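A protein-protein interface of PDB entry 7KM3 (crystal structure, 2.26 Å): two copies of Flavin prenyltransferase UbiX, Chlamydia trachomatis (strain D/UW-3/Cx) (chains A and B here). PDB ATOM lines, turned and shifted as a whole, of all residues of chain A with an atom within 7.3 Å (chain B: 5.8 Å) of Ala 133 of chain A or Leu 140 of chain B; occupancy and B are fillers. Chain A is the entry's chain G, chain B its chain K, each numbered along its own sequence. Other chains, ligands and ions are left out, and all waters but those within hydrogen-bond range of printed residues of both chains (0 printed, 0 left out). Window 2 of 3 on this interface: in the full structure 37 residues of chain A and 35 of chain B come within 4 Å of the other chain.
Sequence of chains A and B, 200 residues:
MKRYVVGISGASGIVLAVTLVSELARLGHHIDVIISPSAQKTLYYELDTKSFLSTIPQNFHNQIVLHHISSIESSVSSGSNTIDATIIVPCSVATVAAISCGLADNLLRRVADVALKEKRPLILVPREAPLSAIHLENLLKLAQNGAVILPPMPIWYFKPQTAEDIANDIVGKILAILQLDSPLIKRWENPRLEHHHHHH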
ATOM      1  N   LEU A 131       5.841 -26.031  14.467  1.00  0.00           N
ATOM      2  CA  LEU A 131       4.817 -26.043  13.429  1.00  0.00           C
ATOM      3  C   LEU A 131       4.576 -24.616  12.971  1.00  0.00           C
ATOM      4  O   LEU A 131       4.146 -23.774  13.762  1.00  0.00           O
ATOM      5  CB  LEU A 131       3.510 -26.635  13.938  1.00  0.00           C
ATOM      6  CG  LEU A 131       3.506 -28.128  14.214  1.00  0.00           C
ATOM      7  CD1 LEU A 131       2.187 -28.496  14.873  1.00  0.00           C
ATOM      8  CD2 LEU A 131       3.684 -28.860  12.883  1.00  0.00           C
ATOM      9  N   SER A 132       4.832 -24.349  11.702  1.00  0.00           N
ATOM     10  CA  SER A 132       4.580 -23.015  11.198  1.00  0.00           C
ATOM     11  C   SER A 132       3.091 -22.806  10.918  1.00  0.00           C
ATOM     12  O   SER A 132       2.288 -23.734  10.956  1.00  0.00           O
ATOM     13  CB  SER A 132       5.368 -22.783   9.926  1.00  0.00           C
ATOM     14  OG  SER A 132       4.866 -23.650   8.947  1.00  0.00           O
ATOM     15  N   ALA A 133       2.748 -21.556  10.602  1.00  0.00           N
ATOM     16  CA  ALA A 133       1.384 -21.203  10.237  1.00  0.00           C
ATOM     17  C   ALA A 133       0.910 -21.999   9.021  1.00  0.00           C
ATOM     18  O   ALA A 133      -0.257 -22.405   8.957  1.00  0.00           O
ATOM     19  CB  ALA A 133       1.300 -19.700   9.959  1.00  0.00           C
ATOM     20  N   ILE A 134       1.809 -22.257   8.068  1.00  0.00           N
ATOM     21  CA  ILE A 134       1.433 -23.046   6.893  1.00  0.00           C
ATOM     22  C   ILE A 134       1.000 -24.452   7.301  1.00  0.00           C
ATOM     23  O   ILE A 134      -0.073 -24.933   6.906  1.00  0.00           O
ATOM     24  CB  ILE A 134       2.587 -23.066   5.874  1.00  0.00           C
ATOM     25  CG1 ILE A 134       2.695 -21.687   5.219  1.00  0.00           C
ATOM     26  CG2 ILE A 134       2.351 -24.151   4.834  1.00  0.00           C
ATOM     27  CD1 ILE A 134       3.874 -21.529   4.303  1.00  0.00           C
ATOM     28  N   HIS A 135       1.804 -25.125   8.125  1.00  0.00           N
ATOM     29  CA  HIS A 135       1.446 -26.487   8.518  1.00  0.00           C
ATOM     30  C   HIS A 135       0.212 -26.510   9.418  1.00  0.00           C
ATOM     31  O   HIS A 135      -0.665 -27.364   9.246  1.00  0.00           O
ATOM     32  CB  HIS A 135       2.664 -27.161   9.155  1.00  0.00           C
ATOM     33  CG  HIS A 135       3.816 -27.262   8.206  1.00  0.00           C
ATOM     34  ND1 HIS A 135       3.702 -27.875   6.969  1.00  0.00           N
ATOM     35  CD2 HIS A 135       5.076 -26.773   8.268  1.00  0.00           C
ATOM     36  CE1 HIS A 135       4.848 -27.772   6.321  1.00  0.00           C
ATOM     37  NE2 HIS A 135       5.700 -27.115   7.089  1.00  0.00           N
ATOM     38  N   LEU A 136       0.081 -25.536  10.320  1.00  0.00           N
ATOM     39  CA  LEU A 136      -1.073 -25.469  11.212  1.00  0.00           C
ATOM     40  C   LEU A 136      -2.373 -25.242  10.433  1.00  0.00           C
ATOM     41  O   LEU A 136      -3.435 -25.745  10.825  1.00  0.00           O
ATOM     42  CB  LEU A 136      -0.875 -24.357  12.248  1.00  0.00           C
ATOM     43  CG  LEU A 136       0.116 -24.669  13.376  1.00  0.00           C
ATOM     44  CD1 LEU A 136       0.556 -23.414  14.181  1.00  0.00           C
ATOM     45  CD2 LEU A 136      -0.452 -25.722  14.301  1.00  0.00           C
ATOM     46  N   GLU A 137      -2.311 -24.458   9.352  1.00  0.00           N
ATOM     47  CA  GLU A 137      -3.488 -24.250   8.526  1.00  0.00           C
ATOM     48  C   GLU A 137      -3.933 -25.559   7.879  1.00  0.00           C
ATOM     49  O   GLU A 137      -5.128 -25.864   7.845  1.00  0.00           O
ATOM     50  CB  GLU A 137      -3.204 -23.182   7.458  1.00  0.00           C
ATOM     51  CG  GLU A 137      -4.363 -22.926   6.542  1.00  0.00           C
ATOM     52  CD  GLU A 137      -4.116 -21.782   5.565  1.00  0.00           C
ATOM     53  OE1 GLU A 137      -3.310 -20.877   5.875  1.00  0.00           O
ATOM     54  OE2 GLU A 137      -4.739 -21.796   4.475  1.00  0.00           O
ATOM     55  N   ASN A 138      -2.979 -26.345   7.380  1.00  0.00           N
ATOM     56  CA  ASN A 138      -3.321 -27.625   6.773  1.00  0.00           C
ATOM     57  C   ASN A 138      -3.911 -28.574   7.814  1.00  0.00           C
ATOM     58  O   ASN A 138      -4.865 -29.318   7.532  1.00  0.00           O
ATOM     59  CB  ASN A 138      -2.085 -28.243   6.102  1.00  0.00           C
ATOM     60  CG  ASN A 138      -1.544 -27.390   4.965  1.00  0.00           C
ATOM     61  OD1 ASN A 138      -2.256 -26.532   4.444  1.00  0.00           O
ATOM     62  ND2 ASN A 138      -0.290 -27.631   4.563  1.00  0.00           N
ATOM     63  N   LEU A 139      -3.363 -28.552   9.028  1.00  0.00           N
ATOM     64  CA  LEU A 139      -3.855 -29.429  10.080  1.00  0.00           C
ATOM     65  C   LEU A 139      -5.279 -29.056  10.458  1.00  0.00           C
ATOM     66  O   LEU A 139      -6.125 -29.940  10.657  1.00  0.00           O
ATOM     67  CB  LEU A 139      -2.935 -29.348  11.300  1.00  0.00           C
ATOM     68  CG  LEU A 139      -1.465 -29.804  11.340  1.00  0.00           C
ATOM     69  CD1 LEU A 139      -0.699 -29.509  12.594  1.00  0.00           C
ATOM     70  CD2 LEU A 139      -1.353 -31.278  10.961  1.00  0.00           C
ATOM     71  N   LEU A 140      -5.559 -27.748  10.539  1.00  0.00           N
ATOM     72  CA  LEU A 140      -6.907 -27.284  10.843  1.00  0.00           C
ATOM     73  C   LEU A 140      -7.887 -27.739   9.772  1.00  0.00           C
ATOM     74  O   LEU A 140      -8.975 -28.240  10.086  1.00  0.00           O
ATOM     75  CB  LEU A 140      -6.922 -25.762  10.983  1.00  0.00           C
ATOM     76  CG  LEU A 140      -8.302 -25.102  11.102  1.00  0.00           C
ATOM     77  CD1 LEU A 140      -9.044 -25.506  12.412  1.00  0.00           C
ATOM     78  CD2 LEU A 140      -8.238 -23.558  10.943  1.00  0.00           C
ATOM     79  N   HIS B 135      -8.672 -26.174  18.906  1.00  0.00           N
ATOM     80  CA  HIS B 135      -7.275 -25.989  19.322  1.00  0.00           C
ATOM     81  C   HIS B 135      -6.389 -25.548  18.165  1.00  0.00           C
ATOM     82  O   HIS B 135      -5.538 -24.665  18.324  1.00  0.00           O
ATOM     83  CB  HIS B 135      -6.681 -27.268  19.896  1.00  0.00           C
ATOM     84  CG  HIS B 135      -7.489 -27.858  20.988  1.00  0.00           C
ATOM     85  ND1 HIS B 135      -7.635 -29.218  21.156  1.00  0.00           N
ATOM     86  CD2 HIS B 135      -8.225 -27.270  21.954  1.00  0.00           C
ATOM     87  CE1 HIS B 135      -8.421 -29.439  22.194  1.00  0.00           C
ATOM     88  NE2 HIS B 135      -8.801 -28.273  22.688  1.00  0.00           N
ATOM     89  N   LEU B 136      -6.526 -26.220  17.020  1.00  0.00           N
ATOM     90  CA  LEU B 136      -5.675 -25.942  15.867  1.00  0.00           C
ATOM     91  C   LEU B 136      -5.849 -24.512  15.379  1.00  0.00           C
ATOM     92  O   LEU B 136      -4.870 -23.855  15.018  1.00  0.00           O
ATOM     93  CB  LEU B 136      -5.972 -26.949  14.747  1.00  0.00           C
ATOM     94  CG  LEU B 136      -5.363 -28.318  15.085  1.00  0.00           C
ATOM     95  CD1 LEU B 136      -5.889 -29.421  14.156  1.00  0.00           C
ATOM     96  CD2 LEU B 136      -3.842 -28.223  15.004  1.00  0.00           C
ATOM     97  N   GLU B 137      -7.086 -24.005  15.395  1.00  0.00           N
ATOM     98  CA  GLU B 137      -7.336 -22.615  15.018  1.00  0.00           C
ATOM     99  C   GLU B 137      -6.686 -21.626  15.988  1.00  0.00           C
ATOM    100  O   GLU B 137      -6.160 -20.598  15.564  1.00  0.00           O
ATOM    101  CB  GLU B 137      -8.850 -22.370  14.915  1.00  0.00           C
ATOM    102  CG  GLU B 137      -9.245 -20.977  14.409  1.00  0.00           C
ATOM    103  CD  GLU B 137     -10.775 -20.764  14.341  1.00  0.00           C
ATOM    104  OE1 GLU B 137     -11.534 -21.748  14.124  1.00  0.00           O
ATOM    105  OE2 GLU B 137     -11.225 -19.610  14.518  1.00  0.00           O
ATOM    106  N   ASN B 138      -6.736 -21.891  17.299  1.00  0.00           N
ATOM    107  CA  ASN B 138      -6.018 -21.010  18.232  1.00  0.00           C
ATOM    108  C   ASN B 138      -4.506 -21.033  17.977  1.00  0.00           C
ATOM    109  O   ASN B 138      -3.846 -19.987  17.995  1.00  0.00           O
ATOM    110  CB  ASN B 138      -6.309 -21.403  19.675  1.00  0.00           C
ATOM    111  CG  ASN B 138      -7.755 -21.153  20.058  1.00  0.00           C
ATOM    112  OD1 ASN B 138      -8.448 -20.352  19.406  1.00  0.00           O
ATOM    113  ND2 ASN B 138      -8.235 -21.858  21.088  1.00  0.00           N
ATOM    114  N   LEU B 139      -3.970 -22.237  17.748  1.00  0.00           N
ATOM    115  CA  LEU B 139      -2.519 -22.416  17.468  1.00  0.00           C
ATOM    116  C   LEU B 139      -2.158 -21.590  16.229  1.00  0.00           C
ATOM    117  O   LEU B 139      -1.239 -20.752  16.323  1.00  0.00           O
ATOM    118  CB  LEU B 139      -2.236 -23.905  17.239  1.00  0.00           C
ATOM    119  CG  LEU B 139      -2.336 -24.790  18.480  1.00  0.00           C
ATOM    120  CD1 LEU B 139      -2.002 -26.236  18.143  1.00  0.00           C
ATOM    121  CD2 LEU B 139      -1.426 -24.278  19.586  1.00  0.00           C
ATOM    122  N   LEU B 140      -2.859 -21.838  15.117  1.00  0.00           N
ATOM    123  CA  LEU B 140      -2.663 -21.111  13.878  1.00  0.00           C
ATOM    124  C   LEU B 140      -2.634 -19.615  14.128  1.00  0.00           C
ATOM    125  O   LEU B 140      -1.705 -18.929  13.705  1.00  0.00           O
ATOM    126  CB  LEU B 140      -3.780 -21.465  12.882  1.00  0.00           C
ATOM    127  CG  LEU B 140      -3.868 -20.617  11.614  1.00  0.00           C
ATOM    128  CD1 LEU B 140      -2.574 -20.743  10.765  1.00  0.00           C
ATOM    129  CD2 LEU B 140      -5.109 -21.045  10.765  1.00  0.00           C
ATOM    130  N   LYS B 141      -3.668 -19.098  14.805  1.00  0.00           N
ATOM    131  CA  LYS B 141      -3.736 -17.678  15.087  1.00  0.00           C
ATOM    132  C   LYS B 141      -2.481 -17.208  15.820  1.00  0.00           C
ATOM    133  O   LYS B 141      -1.920 -16.166  15.477  1.00  0.00           O
ATOM    134  CB  LYS B 141      -4.990 -17.352  15.899  1.00  0.00           C
ATOM    135  CG  LYS B 141      -5.168 -15.834  16.164  1.00  0.00           C
ATOM    136  CD  LYS B 141      -6.440 -15.557  16.961  1.00  0.00           C
ATOM    137  CE  LYS B 141      -6.652 -14.107  17.200  1.00  0.00           C
ATOM    138  NZ  LYS B 141      -7.829 -13.875  18.085  1.00  0.00           N
ATOM    139  N   LEU B 142      -2.025 -17.976  16.820  1.00  0.00           N
ATOM    140  CA  LEU B 142      -0.823 -17.602  17.552  1.00  0.00           C
ATOM    141  C   LEU B 142       0.411 -17.593  16.639  1.00  0.00           C
ATOM    142  O   LEU B 142       1.219 -16.665  16.699  1.00  0.00           O
ATOM    143  CB  LEU B 142      -0.628 -18.538  18.760  1.00  0.00           C
ATOM    144  CG  LEU B 142      -1.617 -18.250  19.901  1.00  0.00           C
ATOM    145  CD1 LEU B 142      -1.686 -19.385  20.923  1.00  0.00           C
ATOM    146  CD2 LEU B 142      -1.259 -16.917  20.578  1.00  0.00           C
ATOM    147  N   ALA B 143       0.542 -18.598  15.762  1.00  0.00           N
ATOM    148  CA  ALA B 143       1.677 -18.623  14.846  1.00  0.00           C
ATOM    149  C   ALA B 143       1.634 -17.441  13.897  1.00  0.00           C
ATOM    150  O   ALA B 143       2.682 -16.855  13.594  1.00  0.00           O
ATOM    151  CB  ALA B 143       1.719 -19.927  14.046  1.00  0.00           C
ATOM    152  N   GLN B 144       0.432 -17.066  13.420  1.00  0.00           N
ATOM    153  CA  GLN B 144       0.342 -15.905  12.539  1.00  0.00           C
ATOM    154  C   GLN B 144       0.745 -14.629  13.255  1.00  0.00           C
ATOM    155  O   GLN B 144       1.182 -13.674  12.608  1.00  0.00           O
ATOM    156  CB  GLN B 144      -1.068 -15.754  11.954  1.00  0.00           C
ATOM    157  CG  GLN B 144      -1.371 -16.775  10.886  1.00  0.00           C
ATOM    158  CD  GLN B 144      -2.866 -16.864  10.553  1.00  0.00           C
ATOM    159  OE1 GLN B 144      -3.725 -16.402  11.305  1.00  0.00           O
ATOM    160  NE2 GLN B 144      -3.171 -17.463   9.428  1.00  0.00           N
ATOM    161  N   ASN B 145       0.600 -14.578  14.577  1.00  0.00           N
ATOM    162  CA  ASN B 145       1.010 -13.396  15.323  1.00  0.00           C
ATOM    163  C   ASN B 145       2.438 -13.481  15.824  1.00  0.00           C
ATOM    164  O   ASN B 145       2.829 -12.635  16.619  1.00  0.00           O
ATOM    165  CB  ASN B 145       0.073 -13.144  16.511  1.00  0.00           C
ATOM    166  CG  ASN B 145      -1.247 -12.534  16.092  1.00  0.00           C
ATOM    167  OD1 ASN B 145      -1.468 -11.346  16.273  1.00  0.00           O
ATOM    168  ND2 ASN B 145      -2.128 -13.353  15.521  1.00  0.00           N
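Ala 133 of chain A touches just these residues of chain B: Leu 140 (3.4 Å) and Ala 143 (3.9 Å). Asn 138 of chain A touches none of the printed residues of chain B. Of the printed residues of chain A, Glu 137 of chain B touches Leu 140 (3.9 Å). Printed residues of chain A within 4 Å of Leu 140 of chain B: Ala 133, Leu 136 and Glu 137. Of the printed residues of chain A, Ala 143 of chain B touches Ala 133 (3.9 Å) and Leu 136 (3.7 Å).
O of Ala 133 of chain A touches CD1 of Leu 140 of chain B (3.4 Å). Ala 133 of chain A touches Ala 143 of chain B (N to CB, 3.9 Å). Leu 136 of chain A touches Leu 139 of chain B. Leu 140 of chain B touches Leu 136 of chain A (N to CD1, 3.9 Å). Ala 143 of chain B touches Leu 136 of chain A (CB to CD1, 3.7 Å). Leu 140 of chain B touches Glu 137 of chain A (CD1 to N, 3.98 Å). O of Leu 139 of chain A touches CD1 of Leu 136 of chain B (3.5 Å). Leu 140 of chain A touches Leu 136 of chain B (N to CD1, 3.999 Å). N of Glu 137 of chain B touches CD1 of Leu 140 of chain A, 3.9 Å away.
Leu 136 of chain A touches Leu 139 of chain B, and with the chains exchanged Leu 139 of chain A touches Leu 136 of chain B. Leu 136 of chain A touches Leu 140 of chain B, and with the chains exchanged Leu 140 of chain A touches Leu 136 of chain B. Glu 137 of chain A touches Leu 140 of chain B, and with the chains exchanged Leu 140 of chain A touches Glu 137 of chain B. Positions printed for both chains: 135, 136, 137, 138, 139 and 140. Of the 9 pairs that touch across the chains among the printed residues, 6 have their exchanged pair printed and touching as well.
Of the 11 printed residues of chain B, 5 touch a printed residue of chain A. Printed residues of chain B that touch a printed residue of chain A: Leu 136, Glu 137, Leu 139, Leu 140 and Ala 143. Among the printed residues, 9 pairs touch across the chains.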
